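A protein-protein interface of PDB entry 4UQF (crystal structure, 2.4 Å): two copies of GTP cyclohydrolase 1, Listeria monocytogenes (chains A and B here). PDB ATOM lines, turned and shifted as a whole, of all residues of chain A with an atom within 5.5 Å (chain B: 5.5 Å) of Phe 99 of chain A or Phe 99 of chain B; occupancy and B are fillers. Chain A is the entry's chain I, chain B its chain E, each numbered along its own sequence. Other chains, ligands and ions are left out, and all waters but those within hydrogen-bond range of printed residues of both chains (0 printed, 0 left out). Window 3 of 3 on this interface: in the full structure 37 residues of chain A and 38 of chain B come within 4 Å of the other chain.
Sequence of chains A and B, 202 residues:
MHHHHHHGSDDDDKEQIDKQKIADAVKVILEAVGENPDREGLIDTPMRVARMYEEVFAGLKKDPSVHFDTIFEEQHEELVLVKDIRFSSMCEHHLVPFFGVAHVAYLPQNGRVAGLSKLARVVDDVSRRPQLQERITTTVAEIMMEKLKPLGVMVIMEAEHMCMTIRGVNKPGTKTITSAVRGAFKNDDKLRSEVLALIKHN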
ATOM      1  N   PHE A  87      19.075  20.948 -17.241  1.00  0.00           N
ATOM      2  CA  PHE A  87      19.531  19.775 -16.507  1.00  0.00           C
ATOM      3  C   PHE A  87      20.635  19.110 -17.301  1.00  0.00           C
ATOM      4  O   PHE A  87      20.789  19.333 -18.497  1.00  0.00           O
ATOM      5  CB  PHE A  87      18.406  18.769 -16.291  1.00  0.00           C
ATOM      6  CG  PHE A  87      18.195  17.863 -17.457  1.00  0.00           C
ATOM      7  CD1 PHE A  87      17.496  18.304 -18.561  1.00  0.00           C
ATOM      8  CD2 PHE A  87      18.718  16.575 -17.463  1.00  0.00           C
ATOM      9  CE1 PHE A  87      17.305  17.479 -19.649  1.00  0.00           C
ATOM     10  CE2 PHE A  87      18.547  15.743 -18.567  1.00  0.00           C
ATOM     11  CZ  PHE A  87      17.832  16.190 -19.650  1.00  0.00           C
ATOM     12  N   SER A  88      21.401  18.283 -16.615  1.00  0.00           N
ATOM     13  CA  SER A  88      22.362  17.421 -17.270  1.00  0.00           C
ATOM     14  C   SER A  88      22.460  16.142 -16.491  1.00  0.00           C
ATOM     15  O   SER A  88      22.091  16.087 -15.333  1.00  0.00           O
ATOM     16  CB  SER A  88      23.727  18.109 -17.390  1.00  0.00           C
ATOM     17  OG  SER A  88      24.173  18.532 -16.126  1.00  0.00           O
ATOM     18  N   SER A  89      22.976  15.118 -17.133  1.00  0.00           N
ATOM     19  CA  SER A  89      23.091  13.822 -16.497  1.00  0.00           C
ATOM     20  C   SER A  89      24.123  13.056 -17.277  1.00  0.00           C
ATOM     21  O   SER A  89      24.745  13.622 -18.156  1.00  0.00           O
ATOM     22  CB  SER A  89      21.724  13.130 -16.555  1.00  0.00           C
ATOM     23  OG  SER A  89      21.700  11.984 -15.753  1.00  0.00           O
ATOM     24  N   PRO A  97      27.904  12.727 -20.895  1.00  0.00           N
ATOM     25  CA  PRO A  97      26.824  13.615 -20.564  1.00  0.00           C
ATOM     26  C   PRO A  97      25.756  13.686 -21.615  1.00  0.00           C
ATOM     27  O   PRO A  97      26.032  13.554 -22.788  1.00  0.00           O
ATOM     28  CB  PRO A  97      27.494  14.983 -20.454  1.00  0.00           C
ATOM     29  CG  PRO A  97      28.910  14.695 -20.168  1.00  0.00           C
ATOM     30  CD  PRO A  97      29.200  13.412 -20.878  1.00  0.00           C
ATOM     31  N   PHE A  98      24.527  13.860 -21.159  1.00  0.00           N
ATOM     32  CA  PHE A  98      23.478  14.411 -21.971  1.00  0.00           C
ATOM     33  C   PHE A  98      22.860  15.576 -21.184  1.00  0.00           C
ATOM     34  O   PHE A  98      22.902  15.603 -19.954  1.00  0.00           O
ATOM     35  CB  PHE A  98      22.473  13.340 -22.403  1.00  0.00           C
ATOM     36  CG  PHE A  98      21.698  12.690 -21.279  1.00  0.00           C
ATOM     37  CD1 PHE A  98      22.201  11.587 -20.605  1.00  0.00           C
ATOM     38  CD2 PHE A  98      20.401  13.075 -21.003  1.00  0.00           C
ATOM     39  CE1 PHE A  98      21.439  10.932 -19.631  1.00  0.00           C
ATOM     40  CE2 PHE A  98      19.654  12.458 -20.028  1.00  0.00           C
ATOM     41  CZ  PHE A  98      20.166  11.376 -19.341  1.00  0.00           C
ATOM     42  N   PHE A  99      22.307  16.537 -21.899  1.00  0.00           N
ATOM     43  CA  PHE A  99      21.879  17.780 -21.276  1.00  0.00           C
ATOM     44  C   PHE A  99      20.819  18.462 -22.119  1.00  0.00           C
ATOM     45  O   PHE A  99      20.716  18.241 -23.330  1.00  0.00           O
ATOM     46  CB  PHE A  99      23.069  18.706 -21.123  1.00  0.00           C
ATOM     47  CG  PHE A  99      23.622  19.156 -22.423  1.00  0.00           C
ATOM     48  CD1 PHE A  99      24.423  18.313 -23.172  1.00  0.00           C
ATOM     49  CD2 PHE A  99      23.274  20.393 -22.958  1.00  0.00           C
ATOM     50  CE1 PHE A  99      24.908  18.706 -24.407  1.00  0.00           C
ATOM     51  CE2 PHE A  99      23.745  20.786 -24.199  1.00  0.00           C
ATOM     52  CZ  PHE A  99      24.564  19.938 -24.922  1.00  0.00           C
ATOM     53  N   GLY A 100      20.014  19.280 -21.471  1.00  0.00           N
ATOM     54  CA  GLY A 100      18.973  20.042 -22.158  1.00  0.00           C
ATOM     55  C   GLY A 100      18.028  20.693 -21.147  1.00  0.00           C
ATOM     56  O   GLY A 100      18.477  21.188 -20.130  1.00  0.00           O
ATOM     57  N   VAL A 101      16.725  20.589 -21.384  1.00  0.00           N
ATOM     58  CA  VAL A 101      15.772  21.204 -20.520  1.00  0.00           C
ATOM     59  C   VAL A 101      14.681  20.255 -20.148  1.00  0.00           C
ATOM     60  O   VAL A 101      14.373  19.310 -20.887  1.00  0.00           O
ATOM     61  CB  VAL A 101      15.124  22.427 -21.205  1.00  0.00           C
ATOM     62  CG1 VAL A 101      16.125  23.590 -21.291  1.00  0.00           C
ATOM     63  CG2 VAL A 101      14.615  22.081 -22.599  1.00  0.00           C
ATOM     64  N   GLU A 158      13.856  17.422 -22.997  1.00  0.00           N
ATOM     65  CA  GLU A 158      14.448  17.566 -24.302  1.00  0.00           C
ATOM     66  C   GLU A 158      15.947  17.651 -24.110  1.00  0.00           C
ATOM     67  O   GLU A 158      16.420  18.457 -23.314  1.00  0.00           O
ATOM     68  CB  GLU A 158      13.927  18.836 -24.927  1.00  0.00           C
ATOM     69  CG  GLU A 158      14.321  18.989 -26.375  1.00  0.00           C
ATOM     70  CD  GLU A 158      13.584  20.110 -27.061  1.00  0.00           C
ATOM     71  OE1 GLU A 158      12.650  20.713 -26.429  1.00  0.00           O
ATOM     72  OE2 GLU A 158      13.957  20.367 -28.230  1.00  0.00           O
ATOM     73  N   ALA A 159      16.703  16.801 -24.791  1.00  0.00           N
ATOM     74  CA  ALA A 159      18.125  16.755 -24.545  1.00  0.00           C
ATOM     75  C   ALA A 159      18.933  16.313 -25.729  1.00  0.00           C
ATOM     76  O   ALA A 159      18.443  15.605 -26.617  1.00  0.00           O
ATOM     77  CB  ALA A 159      18.419  15.835 -23.357  1.00  0.00           C
ATOM     78  N   GLU A 160      20.202  16.707 -25.708  1.00  0.00           N
ATOM     79  CA  GLU A 160      21.160  16.218 -26.663  1.00  0.00           C
ATOM     80  C   GLU A 160      22.086  15.228 -25.957  1.00  0.00           C
ATOM     81  O   GLU A 160      22.491  15.452 -24.821  1.00  0.00           O
ATOM     82  CB  GLU A 160      21.943  17.344 -27.268  1.00  0.00           C
ATOM     83  CG  GLU A 160      22.962  16.867 -28.306  1.00  0.00           C
ATOM     84  CD  GLU A 160      23.553  17.996 -29.144  1.00  0.00           C
ATOM     85  OE1 GLU A 160      22.920  19.085 -29.196  1.00  0.00           O
ATOM     86  OE2 GLU A 160      24.651  17.783 -29.728  1.00  0.00           O
ATOM     87  N   HIS A 161      22.380  14.123 -26.633  1.00  0.00           N
ATOM     88  CA  HIS A 161      23.224  13.077 -26.064  1.00  0.00           C
ATOM     89  C   HIS A 161      24.569  13.074 -26.752  1.00  0.00           C
ATOM     90  O   HIS A 161      24.648  12.938 -27.970  1.00  0.00           O
ATOM     91  CB  HIS A 161      22.562  11.703 -26.232  1.00  0.00           C
ATOM     92  CG  HIS A 161      21.389  11.483 -25.334  1.00  0.00           C
ATOM     93  ND1 HIS A 161      20.179  12.116 -25.501  1.00  0.00           N
ATOM     94  CD2 HIS A 161      21.257  10.707 -24.236  1.00  0.00           C
ATOM     95  CE1 HIS A 161      19.345  11.722 -24.555  1.00  0.00           C
ATOM     96  NE2 HIS A 161      19.978  10.872 -23.772  1.00  0.00           N
ATOM     97  N   MET A 162      25.625  13.207 -25.965  1.00  0.00           N
ATOM     98  CA  MET A 162      26.969  13.045 -26.492  1.00  0.00           C
ATOM     99  C   MET A 162      27.230  11.562 -26.831  1.00  0.00           C
ATOM    100  O   MET A 162      27.984  11.335 -27.758  1.00  0.00           O
ATOM    101  CB  MET A 162      28.011  13.580 -25.507  1.00  0.00           C
ATOM    102  CG  MET A 162      27.760  14.981 -24.948  1.00  0.00           C
ATOM    103  SD  MET A 162      28.275  16.294 -26.049  1.00  0.00           S
ATOM    104  CE  MET A 162      26.787  16.579 -27.003  1.00  0.00           C
ATOM    105  N   THR A 165      26.872  12.282 -30.350  1.00  0.00           N
ATOM    106  CA  THR A 165      27.522  13.374 -31.084  1.00  0.00           C
ATOM    107  C   THR A 165      29.014  13.085 -31.342  1.00  0.00           C
ATOM    108  O   THR A 165      29.557  13.471 -32.356  1.00  0.00           O
ATOM    109  CB  THR A 165      27.346  14.702 -30.307  1.00  0.00           C
ATOM    110  OG1 THR A 165      25.936  15.032 -30.223  1.00  0.00           O
ATOM    111  CG2 THR A 165      28.136  15.827 -30.961  1.00  0.00           C
ATOM    112  N   PHE B  87      33.286  19.564 -34.760  1.00  0.00           N
ATOM    113  CA  PHE B  87      34.250  18.679 -34.170  1.00  0.00           C
ATOM    114  C   PHE B  87      33.838  18.359 -32.760  1.00  0.00           C
ATOM    115  O   PHE B  87      33.026  19.061 -32.162  1.00  0.00           O
ATOM    116  CB  PHE B  87      35.642  19.311 -34.143  1.00  0.00           C
ATOM    117  CG  PHE B  87      35.860  20.210 -32.969  1.00  0.00           C
ATOM    118  CD1 PHE B  87      35.361  21.502 -32.991  1.00  0.00           C
ATOM    119  CD2 PHE B  87      36.536  19.761 -31.839  1.00  0.00           C
ATOM    120  CE1 PHE B  87      35.520  22.352 -31.905  1.00  0.00           C
ATOM    121  CE2 PHE B  87      36.701  20.597 -30.753  1.00  0.00           C
ATOM    122  CZ  PHE B  87      36.195  21.903 -30.789  1.00  0.00           C
ATOM    123  N   SER B  88      34.414  17.300 -32.218  1.00  0.00           N
ATOM    124  CA  SER B  88      34.258  16.990 -30.809  1.00  0.00           C
ATOM    125  C   SER B  88      35.533  16.330 -30.323  1.00  0.00           C
ATOM    126  O   SER B  88      36.318  15.814 -31.094  1.00  0.00           O
ATOM    127  CB  SER B  88      33.053  16.084 -30.551  1.00  0.00           C
ATOM    128  OG  SER B  88      33.147  14.913 -31.325  1.00  0.00           O
ATOM    129  N   SER B  89      35.754  16.368 -29.024  1.00  0.00           N
ATOM    130  CA  SER B  89      36.964  15.798 -28.459  1.00  0.00           C
ATOM    131  C   SER B  89      36.647  15.492 -26.996  1.00  0.00           C
ATOM    132  O   SER B  89      35.507  15.658 -26.595  1.00  0.00           O
ATOM    133  CB  SER B  89      38.088  16.798 -28.620  1.00  0.00           C
ATOM    134  OG  SER B  89      39.333  16.236 -28.266  1.00  0.00           O
ATOM    135  N   PRO B  97      33.370  15.079 -22.998  1.00  0.00           N
ATOM    136  CA  PRO B  97      33.371  15.725 -24.298  1.00  0.00           C
ATOM    137  C   PRO B  97      33.307  17.255 -24.252  1.00  0.00           C
ATOM    138  O   PRO B  97      32.684  17.843 -23.364  1.00  0.00           O
ATOM    139  CB  PRO B  97      32.112  15.205 -24.956  1.00  0.00           C
ATOM    140  CG  PRO B  97      31.790  13.946 -24.229  1.00  0.00           C
ATOM    141  CD  PRO B  97      32.220  14.187 -22.833  1.00  0.00           C
ATOM    142  N   PHE B  98      34.005  17.867 -25.194  1.00  0.00           N
ATOM    143  CA  PHE B  98      33.702  19.225 -25.620  1.00  0.00           C
ATOM    144  C   PHE B  98      33.530  19.208 -27.138  1.00  0.00           C
ATOM    145  O   PHE B  98      34.058  18.328 -27.816  1.00  0.00           O
ATOM    146  CB  PHE B  98      34.739  20.234 -25.122  1.00  0.00           C
ATOM    147  CG  PHE B  98      36.134  20.036 -25.663  1.00  0.00           C
ATOM    148  CD1 PHE B  98      37.017  19.142 -25.080  1.00  0.00           C
ATOM    149  CD2 PHE B  98      36.603  20.815 -26.692  1.00  0.00           C
ATOM    150  CE1 PHE B  98      38.319  19.011 -25.560  1.00  0.00           C
ATOM    151  CE2 PHE B  98      37.897  20.679 -27.173  1.00  0.00           C
ATOM    152  CZ  PHE B  98      38.757  19.780 -26.606  1.00  0.00           C
ATOM    153  N   PHE B  99      32.740  20.142 -27.653  1.00  0.00           N
ATOM    154  CA  PHE B  99      32.335  20.086 -29.048  1.00  0.00           C
ATOM    155  C   PHE B  99      31.964  21.485 -29.544  1.00  0.00           C
ATOM    156  O   PHE B  99      31.540  22.335 -28.754  1.00  0.00           O
ATOM    157  CB  PHE B  99      31.136  19.136 -29.199  1.00  0.00           C
ATOM    158  CG  PHE B  99      29.912  19.636 -28.510  1.00  0.00           C
ATOM    159  CD1 PHE B  99      29.763  19.489 -27.125  1.00  0.00           C
ATOM    160  CD2 PHE B  99      28.931  20.310 -29.208  1.00  0.00           C
ATOM    161  CE1 PHE B  99      28.655  20.003 -26.463  1.00  0.00           C
ATOM    162  CE2 PHE B  99      27.807  20.812 -28.544  1.00  0.00           C
ATOM    163  CZ  PHE B  99      27.674  20.653 -27.175  1.00  0.00           C
ATOM    164  N   GLY B 100      32.071  21.688 -30.852  1.00  0.00           N
ATOM    165  CA  GLY B 100      31.641  22.899 -31.450  1.00  0.00           C
ATOM    166  C   GLY B 100      32.081  22.943 -32.876  1.00  0.00           C
ATOM    167  O   GLY B 100      31.977  21.960 -33.591  1.00  0.00           O
ATOM    168  N   VAL B 101      32.658  24.072 -33.282  1.00  0.00           N
ATOM    169  CA  VAL B 101      33.063  24.240 -34.659  1.00  0.00           C
ATOM    170  C   VAL B 101      34.481  24.724 -34.728  1.00  0.00           C
ATOM    171  O   VAL B 101      34.955  25.425 -33.834  1.00  0.00           O
ATOM    172  CB  VAL B 101      32.148  25.232 -35.407  1.00  0.00           C
ATOM    173  CG1 VAL B 101      30.789  24.619 -35.654  1.00  0.00           C
ATOM    174  CG2 VAL B 101      31.979  26.542 -34.635  1.00  0.00           C
ATOM    175  N   GLU B 158      35.574  27.165 -31.629  1.00  0.00           N
ATOM    176  CA  GLU B 158      34.554  27.614 -30.702  1.00  0.00           C
ATOM    177  C   GLU B 158      33.888  26.379 -30.157  1.00  0.00           C
ATOM    178  O   GLU B 158      33.432  25.523 -30.924  1.00  0.00           O
ATOM    179  CB  GLU B 158      33.584  28.460 -31.446  1.00  0.00           C
ATOM    180  CG  GLU B 158      32.601  29.150 -30.546  1.00  0.00           C
ATOM    181  CD  GLU B 158      31.798  30.223 -31.272  1.00  0.00           C
ATOM    182  OE1 GLU B 158      32.102  30.516 -32.471  1.00  0.00           O
ATOM    183  OE2 GLU B 158      30.866  30.749 -30.619  1.00  0.00           O
ATOM    184  N   ALA B 159      33.870  26.230 -28.841  1.00  0.00           N
ATOM    185  CA  ALA B 159      33.308  25.007 -28.282  1.00  0.00           C
ATOM    186  C   ALA B 159      32.654  25.202 -26.943  1.00  0.00           C
ATOM    187  O   ALA B 159      32.962  26.144 -26.207  1.00  0.00           O
ATOM    188  CB  ALA B 159      34.391  23.945 -28.181  1.00  0.00           C
ATOM    189  N   GLU B 160      31.774  24.252 -26.623  1.00  0.00           N
ATOM    190  CA  GLU B 160      31.188  24.169 -25.305  1.00  0.00           C
ATOM    191  C   GLU B 160      31.792  22.970 -24.606  1.00  0.00           C
ATOM    192  O   GLU B 160      31.991  21.918 -25.199  1.00  0.00           O
ATOM    193  CB  GLU B 160      29.689  24.052 -25.371  1.00  0.00           C
ATOM    194  CG  GLU B 160      29.052  23.985 -23.981  1.00  0.00           C
ATOM    195  CD  GLU B 160      27.545  24.168 -23.993  1.00  0.00           C
ATOM    196  OE1 GLU B 160      27.026  24.717 -24.996  1.00  0.00           O
ATOM    197  OE2 GLU B 160      26.897  23.745 -23.003  1.00  0.00           O
ATOM    198  N   HIS B 161      32.148  23.168 -23.346  1.00  0.00           N
ATOM    199  CA  HIS B 161      32.782  22.126 -22.552  1.00  0.00           C
ATOM    200  C   HIS B 161      31.796  21.594 -21.537  1.00  0.00           C
ATOM    201  O   HIS B 161      31.285  22.359 -20.715  1.00  0.00           O
ATOM    202  CB  HIS B 161      34.013  22.690 -21.843  1.00  0.00           C
ATOM    203  CG  HIS B 161      35.123  23.035 -22.779  1.00  0.00           C
ATOM    204  ND1 HIS B 161      36.315  22.343 -22.809  1.00  0.00           N
ATOM    205  CD2 HIS B 161      35.201  23.957 -23.762  1.00  0.00           C
ATOM    206  CE1 HIS B 161      37.091  22.829 -23.757  1.00  0.00           C
ATOM    207  NE2 HIS B 161      36.441  23.816 -24.346  1.00  0.00           N
ATOM    208  N   MET B 162      31.568  20.288 -21.568  1.00  0.00           N
ATOM    209  CA  MET B 162      30.805  19.646 -20.513  1.00  0.00           C
ATOM    210  C   MET B 162      31.593  19.618 -19.184  1.00  0.00           C
ATOM    211  O   MET B 162      30.957  19.713 -18.154  1.00  0.00           O
ATOM    212  CB  MET B 162      30.398  18.230 -20.927  1.00  0.00           C
ATOM    213  CG  MET B 162      29.766  18.088 -22.301  1.00  0.00           C
ATOM    214  SD  MET B 162      28.004  18.509 -22.326  1.00  0.00           S
ATOM    215  CE  MET B 162      28.047  20.263 -22.706  1.00  0.00           C
ATOM    216  N   THR B 165      29.553  22.294 -17.861  1.00  0.00           N
ATOM    217  CA  THR B 165      28.098  22.358 -17.890  1.00  0.00           C
ATOM    218  C   THR B 165      27.467  21.422 -16.850  1.00  0.00           C
ATOM    219  O   THR B 165      26.426  21.721 -16.285  1.00  0.00           O
ATOM    220  CB  THR B 165      27.588  22.021 -19.317  1.00  0.00           C
ATOM    221  OG1 THR B 165      28.057  23.024 -20.256  1.00  0.00           O
ATOM    222  CG2 THR B 165      26.060  21.927 -19.346  1.00  0.00           C
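Of the 14 printed residues of chain A, 4 touch a printed residue of chain B. Printed residues of chain A that touch a printed residue of chain B: Ser 88, Pro 97, Phe 99 and Met 162. Of the 14 printed residues of chain B, 4 touch a printed residue of chain A. Among the printed residues, no Asp or Glu carboxylate lies within 4 Å of a Lys or Arg side-chain nitrogen of the other chain.
Of the printed residues of chain B, Ser 88 of chain A touches Thr 165 (3.9 Å). Ser 89 of chain A touches none of the printed residues of chain B. Of the printed residues of chain B, Pro 97 of chain A touches Pro 97 (3.7 Å) and Met 162 (3.9 Å). Phe 99 of chain A touches just these residues of chain B: Phe 99 (3.9 Å) and Met 162 (3.7 Å). Of the printed residues of chain B, Met 162 of chain A touches Phe 99. Of the printed residues of chain A, Pro 97 of chain B touches Pro 97. Phe 99 of chain B touches just these residues of chain A: Phe 99 (3.9 Å) and Met 162 (3.7 Å). Printed residues of chain A within 4 Å of Thr 165 of chain B: Ser 88 (3.9 Å). The nearest residue of chain B that does not touch Phe 99 of chain A is Glu 160 of chain B (4.5 Å). The nearest printed residue of chain B that does not touch Pro 97 of chain A is Thr 165 of chain B (7.1 Å).
Among the printed residues, pairs that only touch across the chains: Pro 97 of chain A with Pro 97 of chain B (3.7 Å), Phe 99 of chain A with Met 162 of chain B (3.7 Å), Met 162 of chain A with Phe 99 of chain B (3.7 Å), Phe 99 of chain A with Phe 99 of chain B (3.9 Å), Ser 88 of chain A with Thr 165 of chain B (3.9 Å) and Pro 97 of chain A with Met 162 of chain B (3.9 Å).
N of Met 162 of chain B sits close to O of Pro 97 of chain B (3.2 Å). The backbone carbonyl oxygen (O) of Phe 99 of chain B lies within hydrogen-bond range of the backbone NH (N) of Glu 160 of chain B (2.9 Å). The side-chain carboxylate (OE2) of Glu 160 of chain B sits at hydrogen-bond distance from the side-chain hydroxyl (OG1) of Thr 165 of chain B. O of His 161 of chain B sits at hydrogen-bond distance from OG1 of Thr 165 of chain B (3.3 Å). The backbone carbonyl oxygen of Pro 97 of chain A lies close to the backbone NH of Met 162 of chain A (3.2 Å). The backbone NH of Glu 160 of chain A lies within hydrogen-bond range of the backbone carbonyl oxygen of Phe 99 of chain A (2.9 Å).
Ser 88 of chain A touches Thr 165 of chain B, but with the chains exchanged Thr 165 of chain A does not touch Ser 88 of chain B (4.004 Å). Pro 97 of chain A touches its own counterpart, Pro 97 of chain B. Pro 97 of chain A touches Met 162 of chain B, but with the chains exchanged Met 162 of chain A does not touch Pro 97 of chain B (4.01 Å). Phe 99 of chain B touches its own counterpart, Phe 99 of chain A. Of the 6 pairs that touch across the chains among the printed residues, 4 have their exchanged pair printed and touching as well.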
